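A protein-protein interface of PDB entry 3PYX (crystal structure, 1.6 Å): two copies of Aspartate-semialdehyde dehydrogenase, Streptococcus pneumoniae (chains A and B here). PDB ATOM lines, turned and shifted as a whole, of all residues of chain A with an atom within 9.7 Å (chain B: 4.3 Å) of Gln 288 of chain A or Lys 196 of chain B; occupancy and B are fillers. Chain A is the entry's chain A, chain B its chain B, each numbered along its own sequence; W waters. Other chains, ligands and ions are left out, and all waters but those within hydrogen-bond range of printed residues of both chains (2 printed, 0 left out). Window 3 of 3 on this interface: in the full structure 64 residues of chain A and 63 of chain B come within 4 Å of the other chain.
The side-chain amino group (NZ) of Lys 197 of chain B sits at hydrogen-bond distance from the backbone carbonyl oxygen (O) of His 287 of chain A, 2.8 Å away.
NE2 of Gln 288 of chain A lies close to OD2 of Asp 195 of chain B (3.4 Å).
The backbone NH (N) of Lys 196 of chain B lies within hydrogen-bond range of the side-chain amide oxygen (OE1) of Gln 288 of chain A, at 3.4 Å.
The side-chain amide oxygen (OE1) of Gln 288 of chain A is in hydrogen-bond range of the backbone NH (N) of Lys 197 of chain B (2.9 Å).
O of Gln 288 of chain A lies within hydrogen-bond range of OH of Tyr 199 of chain B, at 2.6 Å.
The side-chain amide oxygen (OE1) of Gln 208 of chain B sits at hydrogen-bond distance from the side-chain amide nitrogen (NE2) of Gln 288 of chain A (3.1 Å).
OH of Tyr 290 of chain A sits at hydrogen-bond distance from OE1 of Gln 208 of chain B.
ND1 of His 287 of chain A lies within hydrogen-bond range of OD2 of Asp 284 of chain A (2.7 Å).
The backbone carbonyl oxygen (O) of Asp 284 of chain A sits at hydrogen-bond distance from the backbone NH (N) of Ile 289 of chain A, 2.9 Å away.
NE2 of Gln 208 of chain B lies within hydrogen-bond range of OD2 of Asp 195 of chain B (2.9 Å).
NZ of Lys 197 of chain B sits close to OH of Tyr 199 of chain B (3.4 Å).
His 287 of chain A touches Tyr 199 of chain B (O to OH, 3.6 Å).
CG of Pro 191 of chain B touches NE2 of Gln 288 of chain A (3.8 Å).
Lys 197 of chain B touches Ile 289 of chain A.
Pro 191 of chain B touches Tyr 290 of chain A.
Tyr 290 of chain A touches Tyr 199 of chain B (OH to CE2, 3.4 Å).
Tyr 199 of chain B touches Gln 292 of chain A.
Of chain B, only Pro 191, Asp 195, Lys 196, Lys 197, Tyr 199 and Gln 208 come within 4 Å of Gln 288 of chain A.
Lys 196 of chain B touches just one residue of chain A: Gln 288 (3.4 Å).
Of chain A, only Gln 288 comes within 4 Å of Asp 195 of chain B.
Of the printed residues of chain A, Pro 191 of chain B touches Gln 288 and Tyr 290.
Printed residues of chain A within 4 Å of Tyr 199 of chain B: His 287 (3.6 Å), Gln 288 (2.6 Å), Tyr 290 (3.4 Å) and Gln 292 (3.4 Å).
Of the printed residues of chain B, His 287 of chain A touches Lys 197 and Tyr 199.
Printed residues of chain B within 4 Å of Ile 289 of chain A: Lys 197 (3.4 Å).
Printed residues of chain B within 4 Å of Tyr 290 of chain A: Pro 191 (3.4 Å), Tyr 199 (3.4 Å) and Gln 208 (2.7 Å).
Gly 305 of chain A touches none of the printed residues of chain B.
Of the 7 printed residues of chain B, 6 touch a printed residue of chain A.
Printed residues of chain B that touch a printed residue of chain A: Pro 191, Asp 195, Lys 196, Lys 197, Tyr 199 and Gln 208.
Hydrophobic or aromatic side chains of chain B within 4 Å of the printed part of chain A: Pro 191 and Tyr 199.
No position is printed for both chains.
Of the 13 pairs that touch across the chains among the printed residues, none has its exchanged pair printed and touching as well.
Water W1 bridges the backbone carbonyl oxygen of Lys 197 of chain B (2.6 Å) and the side-chain amide nitrogen of Gln 288 of chain A (3.4 Å).
Water W2 bridges OD1 of Asp 195 of chain B (2.8 Å) and O of Ala 286 of chain A (3.3 Å).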
ATOM      1  N   GLU A 282     -13.151  19.560 -21.866  1.00  0.00           N
ATOM      2  CA  GLU A 282     -11.925  18.766 -21.839  1.00  0.00           C
ATOM      3  C   GLU A 282     -12.203  17.585 -20.933  1.00  0.00           C
ATOM      4  O   GLU A 282     -11.948  17.644 -19.717  1.00  0.00           O
ATOM      5  CB  GLU A 282     -10.737  19.566 -21.304  1.00  0.00           C
ATOM      6  CG  GLU A 282     -10.181  20.547 -22.294  1.00  0.00           C
ATOM      7  CD  GLU A 282      -8.955  21.282 -21.803  1.00  0.00           C
ATOM      8  OE1 GLU A 282      -8.730  21.421 -20.569  1.00  0.00           O
ATOM      9  OE2 GLU A 282      -8.212  21.770 -22.682  1.00  0.00           O
ATOM     10  N   ASP A 283     -12.724  16.510 -21.524  1.00  0.00           N
ATOM     11  CA  ASP A 283     -13.282  15.413 -20.731  1.00  0.00           C
ATOM     12  C   ASP A 283     -13.200  14.139 -21.556  1.00  0.00           C
ATOM     13  O   ASP A 283     -14.056  13.854 -22.380  1.00  0.00           O
ATOM     14  CB  ASP A 283     -14.735  15.743 -20.343  1.00  0.00           C
ATOM     15  CG  ASP A 283     -15.235  14.932 -19.153  1.00  0.00           C
ATOM     16  OD1 ASP A 283     -14.708  13.830 -18.919  1.00  0.00           O
ATOM     17  OD2 ASP A 283     -16.194  15.392 -18.484  1.00  0.00           O
ATOM     18  N   ASP A 284     -12.120  13.411 -21.350  1.00  0.00           N
ATOM     19  CA  ASP A 284     -11.917  12.145 -22.022  1.00  0.00           C
ATOM     20  C   ASP A 284     -11.062  11.316 -21.092  1.00  0.00           C
ATOM     21  O   ASP A 284      -9.837  11.263 -21.217  1.00  0.00           O
ATOM     22  CB  ASP A 284     -11.225  12.349 -23.378  1.00  0.00           C
ATOM     23  CG  ASP A 284     -10.957  11.030 -24.105  1.00  0.00           C
ATOM     24  OD1 ASP A 284     -11.477   9.962 -23.688  1.00  0.00           O
ATOM     25  OD2 ASP A 284     -10.207  11.069 -25.106  1.00  0.00           O
ATOM     26  N   VAL A 285     -11.725  10.699 -20.123  1.00  0.00           N
ATOM     27  CA  VAL A 285     -11.007  10.023 -19.046  1.00  0.00           C
ATOM     28  C   VAL A 285     -10.216   8.810 -19.532  1.00  0.00           C
ATOM     29  O   VAL A 285      -9.200   8.484 -18.937  1.00  0.00           O
ATOM     30  CB  VAL A 285     -11.910   9.704 -17.826  1.00  0.00           C
ATOM     31  CG1 VAL A 285     -12.417  11.012 -17.247  1.00  0.00           C
ATOM     32  CG2 VAL A 285     -13.071   8.825 -18.215  1.00  0.00           C
ATOM     33  N   ALA A 286     -10.677   8.181 -20.621  1.00  0.00           N
ATOM     34  CA  ALA A 286      -9.939   7.089 -21.260  1.00  0.00           C
ATOM     35  C   ALA A 286      -8.517   7.502 -21.663  1.00  0.00           C
ATOM     36  O   ALA A 286      -7.607   6.657 -21.702  1.00  0.00           O
ATOM     37  CB  ALA A 286     -10.706   6.561 -22.472  1.00  0.00           C
ATOM     38  N   HIS A 287      -8.315   8.793 -21.943  1.00  0.00           N
ATOM     39  CA  HIS A 287      -6.984   9.314 -22.256  1.00  0.00           C
ATOM     40  C   HIS A 287      -6.498  10.316 -21.213  1.00  0.00           C
ATOM     41  O   HIS A 287      -5.649  11.159 -21.494  1.00  0.00           O
ATOM     42  CB  HIS A 287      -6.958   9.904 -23.679  1.00  0.00           C
ATOM     43  CG  HIS A 287      -7.339   8.907 -24.726  1.00  0.00           C
ATOM     44  ND1 HIS A 287      -8.542   8.952 -25.394  1.00  0.00           N
ATOM     45  CD2 HIS A 287      -6.700   7.798 -25.170  1.00  0.00           C
ATOM     46  CE1 HIS A 287      -8.612   7.933 -26.236  1.00  0.00           C
ATOM     47  NE2 HIS A 287      -7.512   7.212 -26.111  1.00  0.00           N
ATOM     48  N   GLN A 288      -7.035  10.191 -19.989  1.00  0.00           N
ATOM     49  CA  GLN A 288      -6.668  11.078 -18.878  1.00  0.00           C
ATOM     50  C   GLN A 288      -6.751  12.558 -19.263  1.00  0.00           C
ATOM     51  O   GLN A 288      -5.849  13.340 -18.957  1.00  0.00           O
ATOM     52  CB  GLN A 288      -5.275  10.762 -18.353  1.00  0.00           C
ATOM     53  CG  GLN A 288      -5.093   9.345 -17.800  1.00  0.00           C
ATOM     54  CD  GLN A 288      -3.631   9.034 -17.588  1.00  0.00           C
ATOM     55  OE1 GLN A 288      -2.992   8.379 -18.432  1.00  0.00           O
ATOM     56  NE2 GLN A 288      -3.062   9.548 -16.503  1.00  0.00           N
ATOM     57  N   ILE A 289      -7.828  12.919 -19.945  1.00  0.00           N
ATOM     58  CA  ILE A 289      -8.053  14.306 -20.334  1.00  0.00           C
ATOM     59  C   ILE A 289      -9.045  14.975 -19.389  1.00  0.00           C
ATOM     60  O   ILE A 289     -10.178  14.525 -19.260  1.00  0.00           O
ATOM     61  CB  ILE A 289      -8.550  14.451 -21.794  1.00  0.00           C
ATOM     62  CG1 ILE A 289      -7.564  13.774 -22.763  1.00  0.00           C
ATOM     63  CG2 ILE A 289      -8.761  15.946 -22.174  1.00  0.00           C
ATOM     64  CD1 ILE A 289      -6.203  14.349 -22.764  1.00  0.00           C
ATOM     65  N   TYR A 290      -8.580  16.047 -18.758  1.00  0.00           N
ATOM     66  CA  TYR A 290      -9.389  16.869 -17.855  1.00  0.00           C
ATOM     67  C   TYR A 290      -8.742  18.254 -17.776  1.00  0.00           C
ATOM     68  O   TYR A 290      -7.568  18.423 -18.103  1.00  0.00           O
ATOM     69  CB  TYR A 290      -9.494  16.211 -16.446  1.00  0.00           C
ATOM     70  CG  TYR A 290      -8.275  15.401 -16.048  1.00  0.00           C
ATOM     71  CD1 TYR A 290      -7.069  16.048 -15.738  1.00  0.00           C
ATOM     72  CD2 TYR A 290      -8.323  14.002 -16.005  1.00  0.00           C
ATOM     73  CE1 TYR A 290      -5.929  15.310 -15.372  1.00  0.00           C
ATOM     74  CE2 TYR A 290      -7.179  13.239 -15.653  1.00  0.00           C
ATOM     75  CZ  TYR A 290      -5.993  13.913 -15.349  1.00  0.00           C
ATOM     76  OH  TYR A 290      -4.861  13.205 -14.995  1.00  0.00           O
ATOM     77  N   PRO A 291      -9.499  19.278 -17.366  1.00  0.00           N
ATOM     78  CA  PRO A 291      -8.899  20.587 -17.228  1.00  0.00           C
ATOM     79  C   PRO A 291      -7.732  20.617 -16.236  1.00  0.00           C
ATOM     80  O   PRO A 291      -7.775  19.926 -15.202  1.00  0.00           O
ATOM     81  CB  PRO A 291     -10.071  21.450 -16.715  1.00  0.00           C
ATOM     82  CG  PRO A 291     -11.302  20.708 -17.214  1.00  0.00           C
ATOM     83  CD  PRO A 291     -10.935  19.281 -17.043  1.00  0.00           C
ATOM     84  N   GLN A 292      -6.695  21.397 -16.556  1.00  0.00           N
ATOM     85  CA  GLN A 292      -5.530  21.580 -15.663  1.00  0.00           C
ATOM     86  C   GLN A 292      -5.129  23.046 -15.604  1.00  0.00           C
ATOM     87  O   GLN A 292      -5.008  23.698 -16.656  1.00  0.00           O
ATOM     88  CB  GLN A 292      -4.322  20.766 -16.160  1.00  0.00           C
ATOM     89  CG  GLN A 292      -4.529  19.262 -16.186  1.00  0.00           C
ATOM     90  CD  GLN A 292      -3.242  18.542 -16.576  1.00  0.00           C
ATOM     91  OE1 GLN A 292      -2.153  18.966 -16.200  1.00  0.00           O
ATOM     92  NE2 GLN A 292      -3.375  17.472 -17.325  1.00  0.00           N
ATOM     93  N   ASN A 295      -2.422  24.172 -17.984  1.00  0.00           N
ATOM     94  CA  ASN A 295      -2.846  24.266 -19.392  1.00  0.00           C
ATOM     95  C   ASN A 295      -3.755  25.452 -19.675  1.00  0.00           C
ATOM     96  O   ASN A 295      -3.790  25.959 -20.802  1.00  0.00           O
ATOM     97  CB  ASN A 295      -3.522  22.972 -19.853  1.00  0.00           C
ATOM     98  CG  ASN A 295      -2.547  21.806 -19.926  1.00  0.00           C
ATOM     99  OD1 ASN A 295      -1.334  22.004 -20.050  1.00  0.00           O
ATOM    100  ND2 ASN A 295      -3.077  20.598 -19.848  1.00  0.00           N
ATOM    101  N   GLY A 305     -14.391  19.511 -17.173  1.00  0.00           N
ATOM    102  CA  GLY A 305     -14.302  18.068 -17.330  1.00  0.00           C
ATOM    103  C   GLY A 305     -14.613  17.373 -16.026  1.00  0.00           C
ATOM    104  O   GLY A 305     -15.286  17.944 -15.147  1.00  0.00           O
ATOM    105  N   ARG A 306     -14.121  16.143 -15.903  1.00  0.00           N
ATOM    106  CA  ARG A 306     -14.530  15.216 -14.831  1.00  0.00           C
ATOM    107  C   ARG A 306     -16.052  15.144 -14.650  1.00  0.00           C
ATOM    108  O   ARG A 306     -16.523  14.926 -13.540  1.00  0.00           O
ATOM    109  CB  ARG A 306     -13.830  15.528 -13.478  1.00  0.00           C
ATOM    110  CG  ARG A 306     -12.274  15.470 -13.439  1.00  0.00           C
ATOM    111  CD  ARG A 306     -11.715  14.028 -13.721  1.00  0.00           C
ATOM    112  NE  ARG A 306     -12.575  12.987 -13.149  1.00  0.00           N
ATOM    113  CZ  ARG A 306     -12.548  12.593 -11.867  1.00  0.00           C
ATOM    114  NH1 ARG A 306     -11.688  13.125 -11.002  1.00  0.00           N
ATOM    115  NH2 ARG A 306     -13.401  11.665 -11.452  1.00  0.00           N
ATOM    116  N   PRO B 191       0.095  11.892 -12.683  1.00  0.00           N
ATOM    117  CA  PRO B 191      -0.768  11.670 -11.507  1.00  0.00           C
ATOM    118  C   PRO B 191      -0.720  10.247 -10.949  1.00  0.00           C
ATOM    119  O   PRO B 191      -0.944  10.057  -9.741  1.00  0.00           O
ATOM    120  CB  PRO B 191      -2.178  11.998 -12.034  1.00  0.00           C
ATOM    121  CG  PRO B 191      -2.095  11.784 -13.538  1.00  0.00           C
ATOM    122  CD  PRO B 191      -0.689  12.188 -13.903  1.00  0.00           C
ATOM    123  N   GLY B 194       1.238   4.020 -12.583  1.00  0.00           N
ATOM    124  CA  GLY B 194       0.849   2.912 -13.462  1.00  0.00           C
ATOM    125  C   GLY B 194       0.116   3.288 -14.742  1.00  0.00           C
ATOM    126  O   GLY B 194       0.105   2.507 -15.711  1.00  0.00           O
ATOM    127  N   ASP B 195      -0.485   4.480 -14.769  1.00  0.00           N
ATOM    128  CA  ASP B 195      -1.294   4.903 -15.909  1.00  0.00           C
ATOM    129  C   ASP B 195      -0.408   5.316 -17.088  1.00  0.00           C
ATOM    130  O   ASP B 195       0.823   5.392 -16.971  1.00  0.00           O
ATOM    131  CB  ASP B 195      -2.253   6.046 -15.499  1.00  0.00           C
ATOM    132  CG  ASP B 195      -3.613   5.947 -16.166  1.00  0.00           C
ATOM    133  OD1 ASP B 195      -3.749   5.260 -17.198  1.00  0.00           O
ATOM    134  OD2 ASP B 195      -4.574   6.581 -15.668  1.00  0.00           O
ATOM    135  N   LYS B 196      -1.054   5.620 -18.207  1.00  0.00           N
ATOM    136  CA  LYS B 196      -0.375   5.741 -19.498  1.00  0.00           C
ATOM    137  C   LYS B 196       0.327   7.078 -19.727  1.00  0.00           C
ATOM    138  O   LYS B 196       1.346   7.142 -20.416  1.00  0.00           O
ATOM    139  CB  LYS B 196      -1.374   5.490 -20.624  1.00  0.00           C
ATOM    140  CG  LYS B 196      -1.964   4.075 -20.624  1.00  0.00           C
ATOM    141  CD  LYS B 196      -2.977   3.911 -21.743  1.00  0.00           C
ATOM    142  CE  LYS B 196      -3.954   2.784 -21.440  1.00  0.00           C
ATOM    143  NZ  LYS B 196      -4.943   2.600 -22.548  1.00  0.00           N
ATOM    144  N   LYS B 197      -0.231   8.148 -19.168  1.00  0.00           N
ATOM    145  CA  LYS B 197       0.265   9.504 -19.391  1.00  0.00           C
ATOM    146  C   LYS B 197       0.608  10.164 -18.060  1.00  0.00           C
ATOM    147  O   LYS B 197      -0.068   9.909 -17.055  1.00  0.00           O
ATOM    148  CB  LYS B 197      -0.793  10.327 -20.134  1.00  0.00           C
ATOM    149  CG  LYS B 197      -1.025   9.826 -21.567  1.00  0.00           C
ATOM    150  CD  LYS B 197      -2.341  10.332 -22.139  1.00  0.00           C
ATOM    151  CE  LYS B 197      -2.259  11.795 -22.510  1.00  0.00           C
ATOM    152  NZ  LYS B 197      -3.566  12.270 -23.072  1.00  0.00           N
ATOM    153  N   TYR B 199       1.753  13.932 -16.025  1.00  0.00           N
ATOM    154  CA  TYR B 199       1.602  15.379 -16.092  1.00  0.00           C
ATOM    155  C   TYR B 199       2.367  16.048 -14.954  1.00  0.00           C
ATOM    156  O   TYR B 199       2.542  15.434 -13.891  1.00  0.00           O
ATOM    157  CB  TYR B 199       0.113  15.734 -15.986  1.00  0.00           C
ATOM    158  CG  TYR B 199      -0.795  15.115 -17.034  1.00  0.00           C
ATOM    159  CD1 TYR B 199      -0.542  15.276 -18.417  1.00  0.00           C
ATOM    160  CD2 TYR B 199      -1.949  14.421 -16.663  1.00  0.00           C
ATOM    161  CE1 TYR B 199      -1.392  14.726 -19.373  1.00  0.00           C
ATOM    162  CE2 TYR B 199      -2.815  13.880 -17.611  1.00  0.00           C
ATOM    163  CZ  TYR B 199      -2.526  14.027 -18.978  1.00  0.00           C
ATOM    164  OH  TYR B 199      -3.402  13.494 -19.912  1.00  0.00           O
ATOM    165  N   GLN B 208      -6.931  13.690 -10.706  1.00  0.00           N
ATOM    166  CA  GLN B 208      -6.804  12.265 -10.892  1.00  0.00           C
ATOM    167  C   GLN B 208      -5.847  11.712  -9.842  1.00  0.00           C
ATOM    168  O   GLN B 208      -4.676  12.123  -9.757  1.00  0.00           O
ATOM    169  CB  GLN B 208      -6.232  11.902 -12.284  1.00  0.00           C
ATOM    170  CG  GLN B 208      -6.209  10.379 -12.427  1.00  0.00           C
ATOM    171  CD  GLN B 208      -5.492   9.865 -13.674  1.00  0.00           C
ATOM    172  OE1 GLN B 208      -5.235  10.606 -14.628  1.00  0.00           O
ATOM    173  NE2 GLN B 208      -5.192   8.577 -13.670  1.00  0.00           N
HETATM  174  O   HOH W   1      -0.322   9.093 -14.595  1.00  0.00           O
HETATM  175  O   HOH W   2      -5.539   5.538 -19.381  1.00  0.00           O
